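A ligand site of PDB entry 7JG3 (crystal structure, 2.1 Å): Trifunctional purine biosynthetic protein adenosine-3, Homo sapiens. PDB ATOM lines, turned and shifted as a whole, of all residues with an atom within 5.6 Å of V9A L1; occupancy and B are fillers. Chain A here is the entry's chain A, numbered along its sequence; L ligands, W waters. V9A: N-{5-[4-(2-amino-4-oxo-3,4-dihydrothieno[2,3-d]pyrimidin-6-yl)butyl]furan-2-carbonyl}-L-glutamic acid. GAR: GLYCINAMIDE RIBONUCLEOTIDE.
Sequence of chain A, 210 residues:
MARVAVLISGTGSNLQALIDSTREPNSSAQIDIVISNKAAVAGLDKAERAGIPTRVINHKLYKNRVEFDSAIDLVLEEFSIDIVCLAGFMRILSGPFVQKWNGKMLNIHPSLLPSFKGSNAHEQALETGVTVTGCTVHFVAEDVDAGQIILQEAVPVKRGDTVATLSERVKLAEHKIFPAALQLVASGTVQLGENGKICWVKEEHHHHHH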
ATOM      1  N   LYS A  38     -15.621   8.489 -13.841  1.00  0.00           N
ATOM      2  CA  LYS A  38     -16.170   9.661 -13.163  1.00  0.00           C
ATOM      3  C   LYS A  38     -17.455   9.265 -12.447  1.00  0.00           C
ATOM      4  O   LYS A  38     -18.334   8.650 -13.046  1.00  0.00           O
ATOM      5  CB  LYS A  38     -16.440  10.792 -14.161  1.00  0.00           C
ATOM      6  CG  LYS A  38     -15.184  11.447 -14.707  1.00  0.00           C
ATOM      7  CD  LYS A  38     -15.484  12.307 -15.928  1.00  0.00           C
ATOM      8  CE  LYS A  38     -14.216  12.945 -16.483  1.00  0.00           C
ATOM      9  NZ  LYS A  38     -14.443  13.567 -17.820  1.00  0.00           N
ATOM     10  N   ARG A  65      -1.068   6.309 -16.195  1.00  0.00           N
ATOM     11  CA  ARG A  65      -2.101   5.587 -16.915  1.00  0.00           C
ATOM     12  C   ARG A  65      -2.005   4.091 -16.674  1.00  0.00           C
ATOM     13  O   ARG A  65      -3.032   3.404 -16.580  1.00  0.00           O
ATOM     14  CB  ARG A  65      -2.034   5.894 -18.417  1.00  0.00           C
ATOM     15  CG  ARG A  65      -2.603   7.237 -18.772  1.00  0.00           C
ATOM     16  CD  ARG A  65      -2.518   7.507 -20.271  1.00  0.00           C
ATOM     17  NE  ARG A  65      -2.517   8.943 -20.561  1.00  0.00           N
ATOM     18  CZ  ARG A  65      -3.600   9.663 -20.854  1.00  0.00           C
ATOM     19  NH1 ARG A  65      -4.808   9.093 -20.904  1.00  0.00           N
ATOM     20  NH2 ARG A  65      -3.479  10.962 -21.094  1.00  0.00           N
ATOM     21  N   LEU A  86     -15.918   0.929 -25.386  1.00  0.00           N
ATOM     22  CA  LEU A  86     -15.701   2.304 -24.940  1.00  0.00           C
ATOM     23  C   LEU A  86     -16.861   3.140 -25.466  1.00  0.00           C
ATOM     24  O   LEU A  86     -16.978   3.371 -26.663  1.00  0.00           O
ATOM     25  CB  LEU A  86     -14.349   2.825 -25.440  1.00  0.00           C
ATOM     26  CG  LEU A  86     -13.138   1.955 -25.150  1.00  0.00           C
ATOM     27  CD1 LEU A  86     -11.859   2.717 -25.441  1.00  0.00           C
ATOM     28  CD2 LEU A  86     -13.145   1.471 -23.688  1.00  0.00           C
ATOM     29  N   PHE A  89     -16.186   6.905 -23.207  1.00  0.00           N
ATOM     30  CA  PHE A  89     -15.011   6.891 -22.346  1.00  0.00           C
ATOM     31  C   PHE A  89     -13.958   7.803 -22.940  1.00  0.00           C
ATOM     32  O   PHE A  89     -13.567   7.649 -24.100  1.00  0.00           O
ATOM     33  CB  PHE A  89     -14.492   5.461 -22.220  1.00  0.00           C
ATOM     34  CG  PHE A  89     -13.436   5.277 -21.182  1.00  0.00           C
ATOM     35  CD1 PHE A  89     -13.763   5.317 -19.837  1.00  0.00           C
ATOM     36  CD2 PHE A  89     -12.117   5.072 -21.546  1.00  0.00           C
ATOM     37  CE1 PHE A  89     -12.784   5.148 -18.869  1.00  0.00           C
ATOM     38  CE2 PHE A  89     -11.132   4.906 -20.585  1.00  0.00           C
ATOM     39  CZ  PHE A  89     -11.463   4.934 -19.248  1.00  0.00           C
ATOM     40  N   MET A  90     -13.492   8.768 -22.155  1.00  0.00           N
ATOM     41  CA  MET A  90     -12.700   9.860 -22.710  1.00  0.00           C
ATOM     42  C   MET A  90     -11.225   9.794 -22.317  1.00  0.00           C
ATOM     43  O   MET A  90     -10.494  10.754 -22.570  1.00  0.00           O
ATOM     44  CB  MET A  90     -13.295  11.214 -22.300  1.00  0.00           C
ATOM     45  CG  MET A  90     -14.637  11.533 -22.937  1.00  0.00           C
ATOM     46  SD  MET A  90     -14.738  11.136 -24.722  1.00  0.00           S
ATOM     47  CE  MET A  90     -13.650  12.394 -25.408  1.00  0.00           C
ATOM     48  N   ARG A  91     -10.774   8.704 -21.704  1.00  0.00           N
ATOM     49  CA  ARG A  91      -9.373   8.556 -21.346  1.00  0.00           C
ATOM     50  C   ARG A  91      -8.645   7.762 -22.427  1.00  0.00           C
ATOM     51  O   ARG A  91      -9.157   6.777 -22.938  1.00  0.00           O
ATOM     52  CB  ARG A  91      -9.207   7.843 -20.009  1.00  0.00           C
ATOM     53  CG  ARG A  91      -9.903   8.547 -18.866  1.00  0.00           C
ATOM     54  CD  ARG A  91      -9.281   9.899 -18.646  1.00  0.00           C
ATOM     55  NE  ARG A  91      -7.891   9.775 -18.249  1.00  0.00           N
ATOM     56  CZ  ARG A  91      -7.088  10.811 -18.004  1.00  0.00           C
ATOM     57  NH1 ARG A  91      -7.563  12.054 -18.119  1.00  0.00           N
ATOM     58  NH2 ARG A  91      -5.829  10.620 -17.642  1.00  0.00           N
ATOM     59  N   ILE A  92      -7.457   8.207 -22.768  1.00  0.00           N
ATOM     60  CA  ILE A  92      -6.601   7.409 -23.641  1.00  0.00           C
ATOM     61  C   ILE A  92      -5.978   6.267 -22.828  1.00  0.00           C
ATOM     62  O   ILE A  92      -5.539   6.444 -21.697  1.00  0.00           O
ATOM     63  CB  ILE A  92      -5.525   8.282 -24.296  1.00  0.00           C
ATOM     64  CG1 ILE A  92      -6.207   9.301 -25.212  1.00  0.00           C
ATOM     65  CG2 ILE A  92      -4.578   7.422 -25.105  1.00  0.00           C
ATOM     66  CD1 ILE A  92      -5.264  10.344 -25.757  1.00  0.00           C
ATOM     67  N   LEU A  93      -5.983   5.085 -23.410  1.00  0.00           N
ATOM     68  CA  LEU A  93      -5.530   3.884 -22.727  1.00  0.00           C
ATOM     69  C   LEU A  93      -4.085   3.612 -23.093  1.00  0.00           C
ATOM     70  O   LEU A  93      -3.629   3.933 -24.183  1.00  0.00           O
ATOM     71  CB  LEU A  93      -6.425   2.706 -23.093  1.00  0.00           C
ATOM     72  CG  LEU A  93      -7.868   2.971 -22.649  1.00  0.00           C
ATOM     73  CD1 LEU A  93      -8.840   2.019 -23.306  1.00  0.00           C
ATOM     74  CD2 LEU A  93      -7.971   2.860 -21.123  1.00  0.00           C
ATOM     75  N   SER A  94      -3.353   3.013 -22.138  1.00  0.00           N
ATOM     76  CA  SER A  94      -1.935   2.748 -22.338  1.00  0.00           C
ATOM     77  C   SER A  94      -1.722   1.600 -23.330  1.00  0.00           C
ATOM     78  O   SER A  94      -2.570   0.723 -23.516  1.00  0.00           O
ATOM     79  CB  SER A  94      -1.276   2.405 -21.009  1.00  0.00           C
ATOM     80  OG  SER A  94      -1.840   1.223 -20.447  1.00  0.00           O
ATOM     81  N   VAL A  98      -3.980  -1.709 -24.341  1.00  0.00           N
ATOM     82  CA  VAL A  98      -4.538  -1.838 -25.685  1.00  0.00           C
ATOM     83  C   VAL A  98      -4.074  -3.134 -26.327  1.00  0.00           C
ATOM     84  O   VAL A  98      -4.862  -3.842 -26.977  1.00  0.00           O
ATOM     85  CB  VAL A  98      -4.152  -0.608 -26.533  1.00  0.00           C
ATOM     86  CG1 VAL A  98      -4.548  -0.811 -27.997  1.00  0.00           C
ATOM     87  CG2 VAL A  98      -4.787   0.653 -25.948  1.00  0.00           C
ATOM     88  N   ASN A 107     -14.538   1.016 -29.851  1.00  0.00           N
ATOM     89  CA  ASN A 107     -14.793   2.405 -29.501  1.00  0.00           C
ATOM     90  C   ASN A 107     -15.745   2.998 -30.541  1.00  0.00           C
ATOM     91  O   ASN A 107     -15.676   2.654 -31.719  1.00  0.00           O
ATOM     92  CB  ASN A 107     -13.493   3.202 -29.457  1.00  0.00           C
ATOM     93  CG  ASN A 107     -13.723   4.674 -29.231  1.00  0.00           C
ATOM     94  OD1 ASN A 107     -14.299   5.080 -28.213  1.00  0.00           O
ATOM     95  ND2 ASN A 107     -13.290   5.488 -30.184  1.00  0.00           N
ATOM     96  N   ILE A 108     -16.649   3.875 -30.078  1.00  0.00           N
ATOM     97  CA  ILE A 108     -17.528   4.652 -30.956  1.00  0.00           C
ATOM     98  C   ILE A 108     -16.937   6.049 -31.064  1.00  0.00           C
ATOM     99  O   ILE A 108     -16.580   6.675 -30.057  1.00  0.00           O
ATOM    100  CB  ILE A 108     -18.978   4.696 -30.420  1.00  0.00           C
ATOM    101  CG1 ILE A 108     -19.909   5.544 -31.316  1.00  0.00           C
ATOM    102  CG2 ILE A 108     -19.051   5.277 -29.004  1.00  0.00           C
ATOM    103  CD1 ILE A 108     -20.329   4.907 -32.616  1.00  0.00           C
ATOM    104  N   GLY A 118      -9.770  12.608 -32.615  1.00  0.00           N
ATOM    105  CA  GLY A 118      -9.629  13.402 -31.419  1.00  0.00           C
ATOM    106  C   GLY A 118     -10.965  13.687 -30.749  1.00  0.00           C
ATOM    107  O   GLY A 118     -12.015  13.154 -31.112  1.00  0.00           O
ATOM    108  N   SER A 119     -10.912  14.570 -29.766  1.00  0.00           N
ATOM    109  CA  SER A 119     -11.965  14.688 -28.779  1.00  0.00           C
ATOM    110  C   SER A 119     -13.081  15.659 -29.157  1.00  0.00           C
ATOM    111  O   SER A 119     -14.112  15.678 -28.479  1.00  0.00           O
ATOM    112  CB  SER A 119     -11.370  15.132 -27.431  1.00  0.00           C
ATOM    113  OG  SER A 119     -10.749  16.395 -27.587  1.00  0.00           O
ATOM    114  N   HIS A 138     -14.821   1.209 -34.197  1.00  0.00           N
ATOM    115  CA  HIS A 138     -13.577   0.588 -34.619  1.00  0.00           C
ATOM    116  C   HIS A 138     -12.949  -0.178 -33.459  1.00  0.00           C
ATOM    117  O   HIS A 138     -13.216   0.085 -32.282  1.00  0.00           O
ATOM    118  CB  HIS A 138     -12.595   1.650 -35.138  1.00  0.00           C
ATOM    119  CG  HIS A 138     -12.247   2.670 -34.110  1.00  0.00           C
ATOM    120  ND1 HIS A 138     -11.072   2.605 -33.374  1.00  0.00           N
ATOM    121  CD2 HIS A 138     -12.897   3.774 -33.683  1.00  0.00           C
ATOM    122  CE1 HIS A 138     -11.022   3.650 -32.550  1.00  0.00           C
ATOM    123  NE2 HIS A 138     -12.123   4.362 -32.713  1.00  0.00           N
ATOM    124  N   VAL A 140     -10.073  -0.712 -30.985  1.00  0.00           N
ATOM    125  CA  VAL A 140      -9.102   0.218 -30.430  1.00  0.00           C
ATOM    126  C   VAL A 140      -7.696  -0.294 -30.710  1.00  0.00           C
ATOM    127  O   VAL A 140      -7.310  -1.387 -30.269  1.00  0.00           O
ATOM    128  CB  VAL A 140      -9.330   0.408 -28.927  1.00  0.00           C
ATOM    129  CG1 VAL A 140      -8.211   1.254 -28.335  1.00  0.00           C
ATOM    130  CG2 VAL A 140     -10.693   1.012 -28.688  1.00  0.00           C
ATOM    131  N   ALA A 141      -6.937   0.473 -31.470  1.00  0.00           N
ATOM    132  CA  ALA A 141      -5.506   0.227 -31.613  1.00  0.00           C
ATOM    133  C   ALA A 141      -4.733   1.224 -30.755  1.00  0.00           C
ATOM    134  O   ALA A 141      -5.304   2.136 -30.158  1.00  0.00           O
ATOM    135  CB  ALA A 141      -5.083   0.323 -33.085  1.00  0.00           C
ATOM    136  N   GLU A 142      -3.427   1.024 -30.690  1.00  0.00           N
ATOM    137  CA  GLU A 142      -2.623   1.954 -29.898  1.00  0.00           C
ATOM    138  C   GLU A 142      -2.678   3.351 -30.499  1.00  0.00           C
ATOM    139  O   GLU A 142      -2.781   4.339 -29.778  1.00  0.00           O
ATOM    140  CB  GLU A 142      -1.196   1.441 -29.802  1.00  0.00           C
ATOM    141  CG  GLU A 142      -0.452   1.988 -28.618  1.00  0.00           C
ATOM    142  CD  GLU A 142       0.828   1.226 -28.355  1.00  0.00           C
ATOM    143  OE1 GLU A 142       0.785  -0.026 -28.354  1.00  0.00           O
ATOM    144  OE2 GLU A 142       1.879   1.881 -28.162  1.00  0.00           O
ATOM    145  N   ASP A 143      -2.613   3.441 -31.823  1.00  0.00           N
ATOM    146  CA  ASP A 143      -2.776   4.709 -32.516  1.00  0.00           C
ATOM    147  C   ASP A 143      -4.222   5.193 -32.383  1.00  0.00           C
ATOM    148  O   ASP A 143      -5.146   4.533 -32.874  1.00  0.00           O
ATOM    149  CB  ASP A 143      -2.394   4.531 -33.983  1.00  0.00           C
ATOM    150  CG  ASP A 143      -2.036   5.828 -34.645  1.00  0.00           C
ATOM    151  OD1 ASP A 143      -1.796   6.814 -33.915  1.00  0.00           O
ATOM    152  OD2 ASP A 143      -1.985   5.864 -35.894  1.00  0.00           O
ATOM    153  N   VAL A 144      -4.415   6.339 -31.721  1.00  0.00           N
ATOM    154  CA  VAL A 144      -5.755   6.756 -31.340  1.00  0.00           C
ATOM    155  C   VAL A 144      -6.627   6.994 -32.570  1.00  0.00           C
ATOM    156  O   VAL A 144      -6.194   7.611 -33.552  1.00  0.00           O
ATOM    157  CB  VAL A 144      -5.703   8.005 -30.445  1.00  0.00           C
ATOM    158  CG1 VAL A 144      -7.082   8.671 -30.356  1.00  0.00           C
ATOM    159  CG2 VAL A 144      -5.207   7.649 -29.066  1.00  0.00           C
ATOM    160  N   ASP A 145      -7.865   6.477 -32.508  1.00  0.00           N
ATOM    161  CA  ASP A 145      -8.853   6.602 -33.592  1.00  0.00           C
ATOM    162  C   ASP A 145      -8.306   6.093 -34.921  1.00  0.00           C
ATOM    163  O   ASP A 145      -8.648   6.600 -35.991  1.00  0.00           O
ATOM    164  CB  ASP A 145      -9.342   8.053 -33.727  1.00  0.00           C
ATOM    165  CG  ASP A 145     -10.078   8.547 -32.502  1.00  0.00           C
ATOM    166  OD1 ASP A 145     -10.604   7.702 -31.727  1.00  0.00           O
ATOM    167  OD2 ASP A 145     -10.143   9.788 -32.301  1.00  0.00           O
ATOM    168  N   ALA A 146      -7.443   5.068 -34.871  1.00  0.00           N
ATOM    169  CA  ALA A 146      -6.851   4.495 -36.065  1.00  0.00           C
ATOM    170  C   ALA A 146      -6.929   2.964 -36.095  1.00  0.00           C
ATOM    171  O   ALA A 146      -6.412   2.363 -37.028  1.00  0.00           O
ATOM    172  CB  ALA A 146      -5.384   4.943 -36.219  1.00  0.00           C
ATOM    173  N   GLY A 147      -7.566   2.337 -35.109  1.00  0.00           N
ATOM    174  CA  GLY A 147      -7.814   0.916 -35.185  1.00  0.00           C
ATOM    175  C   GLY A 147      -8.760   0.576 -36.328  1.00  0.00           C
ATOM    176  O   GLY A 147      -9.364   1.434 -36.970  1.00  0.00           O
HETATM  177  O25 V9A L   1     -12.515  14.329 -21.508  1.00  0.00           O
HETATM  178  C26 V9A L   1      -6.909  11.947 -21.894  1.00  0.00           C
HETATM  179  C30 V9A L   1     -11.908   5.896 -26.422  1.00  0.00           C
HETATM  180  C32 V9A L   1     -11.110   8.114 -27.198  1.00  0.00           C
HETATM  181  C31 V9A L   1     -12.314   7.177 -27.132  1.00  0.00           C
HETATM  182  C33 V9A L   1     -11.532   9.479 -26.697  1.00  0.00           C
HETATM  183  C20 V9A L   1      -7.860  12.942 -22.543  1.00  0.00           C
HETATM  184  C16 V9A L   1     -10.405  10.491 -26.799  1.00  0.00           C
HETATM  185  C17 V9A L   1      -8.177  12.629 -24.977  1.00  0.00           C
HETATM  186  C22 V9A L   1     -10.234  13.816 -22.186  1.00  0.00           C
HETATM  187  C21 V9A L   1      -8.955  13.298 -21.535  1.00  0.00           C
HETATM  188  C13 V9A L   1      -8.938  11.877 -26.060  1.00  0.00           C
HETATM  189  C8  V9A L   1      -8.515   4.965 -27.958  1.00  0.00           C
HETATM  190  C9  V9A L   1      -7.952   5.017 -26.677  1.00  0.00           C
HETATM  191  C4  V9A L   1      -7.640   4.633 -29.028  1.00  0.00           C
HETATM  192  C14 V9A L   1      -8.798  11.923 -27.459  1.00  0.00           C
HETATM  193  C15 V9A L   1      -9.789  11.001 -27.948  1.00  0.00           C
HETATM  194  C2  V9A L   1      -5.929   4.455 -27.540  1.00  0.00           C
HETATM  195  C23 V9A L   1     -11.302  14.188 -21.151  1.00  0.00           C
HETATM  196  C6  V9A L   1     -10.490   5.557 -26.726  1.00  0.00           C
HETATM  197  C7  V9A L   1      -9.951   5.280 -27.995  1.00  0.00           C
HETATM  198  N1  V9A L   1      -6.660   4.756 -26.458  1.00  0.00           N
HETATM  199  N11 V9A L   1      -4.633   4.206 -27.328  1.00  0.00           N
HETATM  200  N19 V9A L   1      -8.479  12.336 -23.701  1.00  0.00           N
HETATM  201  N3  V9A L   1      -6.344   4.384 -28.815  1.00  0.00           N
HETATM  202  O10 V9A L   1      -8.107   4.588 -30.189  1.00  0.00           O
HETATM  203  O12 V9A L   1      -9.880  11.038 -25.750  1.00  0.00           O
HETATM  204  O18 V9A L   1      -7.326  13.481 -25.263  1.00  0.00           O
HETATM  205  O24 V9A L   1     -10.977  14.344 -19.947  1.00  0.00           O
HETATM  206  O27 V9A L   1      -6.267  12.273 -20.694  1.00  0.00           O
HETATM  207  O28 V9A L   1      -6.669  10.693 -22.476  1.00  0.00           O
HETATM  208  S5  V9A L   1      -9.200   5.432 -25.572  1.00  0.00           S
HETATM  209  C1  GAR L   2     -20.661  10.045 -28.133  1.00  0.00           C
HETATM  210  O6  GAR L   2     -21.201  10.991 -29.039  1.00  0.00           O
HETATM  211  C2  GAR L   2     -19.313   9.555 -28.705  1.00  0.00           C
HETATM  212  O8  GAR L   2     -19.314   9.527 -30.109  1.00  0.00           O
HETATM  213  C3  GAR L   2     -18.302  10.542 -28.071  1.00  0.00           C
HETATM  214  O4  GAR L   2     -18.891  10.908 -26.798  1.00  0.00           O
HETATM  215  C5  GAR L   2     -20.326  10.726 -26.792  1.00  0.00           C
HETATM  216  C10 GAR L   2     -20.799   9.937 -25.584  1.00  0.00           C
HETATM  217  O12 GAR L   2     -22.226   9.990 -25.492  1.00  0.00           O
HETATM  218  N19 GAR L   2     -16.957  10.057 -27.873  1.00  0.00           N
HETATM  219  C21 GAR L   2     -15.921  10.720 -28.432  1.00  0.00           C
HETATM  220  O22 GAR L   2     -15.982  11.853 -28.930  1.00  0.00           O
HETATM  221  C23 GAR L   2     -14.619   9.955 -28.392  1.00  0.00           C
HETATM  222  N24 GAR L   2     -13.488  10.713 -28.883  1.00  0.00           N
HETATM  223  P15 GAR L   2     -22.981   9.046 -24.417  1.00  0.00           P
HETATM  224  O16 GAR L   2     -22.861   7.666 -25.046  1.00  0.00           O
HETATM  225  O17 GAR L   2     -24.393   9.598 -24.340  1.00  0.00           O
HETATM  226  O18 GAR L   2     -22.182   9.244 -23.148  1.00  0.00           O
HETATM  227  O   HOH W   1     -15.291  12.999 -20.477  1.00  0.00           O
HETATM  228  O   HOH W   2     -12.520  11.445 -19.339  1.00  0.00           O
HETATM  229  O   HOH W   3     -15.044   6.200 -25.718  1.00  0.00           O
HETATM  230  O   HOH W   4      -1.682   4.741 -25.754  1.00  0.00           O
HETATM  231  O   HOH W   5      -7.384   3.268 -32.226  1.00  0.00           O
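N11 of V9A L1 sits at hydrogen-bond distance from O of Leu 93 (3.3 Å).
The guanidinium group (NH1) of Arg 91 lies within salt-bridge range of an oxygen (O27) of V9A L1 (2.9 Å).
The backbone NH (N) of Asp 145 sits at hydrogen-bond distance from an oxygen (O10) of V9A L1.
O28 of V9A L1 lies within salt-bridge range of NH1 of Arg 65.
N1 of V9A L1 lies within hydrogen-bond range of N of Leu 93.
A nitrogen (N3) of V9A L1 lies within hydrogen-bond range of the backbone carbonyl oxygen (O) of Ala 141 (2.8 Å).
An oxygen (O28) of V9A L1 is in hydrogen-bond range of the backbone NH (N) of Ile 92 (2.6 Å).
The backbone carbonyl oxygen (O) of Met 90 is in hydrogen-bond range of a nitrogen (N19) of V9A L1 (2.8 Å).
A nitrogen (N11) of V9A L1 lies within hydrogen-bond range of the backbone carbonyl oxygen of Glu 142 (3.1 Å).
N of Gly 118 lies within hydrogen-bond range of OD2 of Asp 145 (2.9 Å).
The backbone NH (N) of Asn 107 sits at hydrogen-bond distance from the backbone carbonyl oxygen (O) of His 138 (2.9 Å).
O of Ile 92 lies within hydrogen-bond range of NH1 of Arg 65.
N of Ile 108 is in hydrogen-bond range of O of Leu 86 (3.5 Å).
Merely in contact with V9A L1: Asn 107, Phe 89, Leu 86, Val 144, Val 140, Val 98, His 138 and Asp 143.
Hydrophobic or aromatic side chains within 4 Å of V9A L1: Leu 86, Met 90, Ile 92, Leu 93, Val 98, His 138, Val 140 and Val 144.
16 residues have an atom within 4 Å of V9A L1: Arg 65, Leu 86, Phe 89, Met 90, Arg 91, Ile 92, Leu 93, Val 98, Asn 107, His 138, Val 140, Ala 141, Glu 142, Asp 143, Val 144 and Asp 145.
The nearest printed residue that does not touch V9A L1 is Gly 118 (4.1 Å).
Water W3 bridges the backbone carbonyl oxygen of Phe 89 and the side-chain amide oxygen of Asn 107.
Water W1 lies within hydrogen-bond range of NZ of Lys 38 (2.8 Å) and O25 of V9A L1 (3.2 Å).
Water W2 lies within hydrogen-bond range of the side-chain amino group (NZ) of Lys 38 and an oxygen (O24) of V9A L1.
Water W4 bridges the backbone carbonyl oxygen (O) of Leu 93 (2.6 Å) and a nitrogen (N11) of V9A L1 (3.4 Å).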
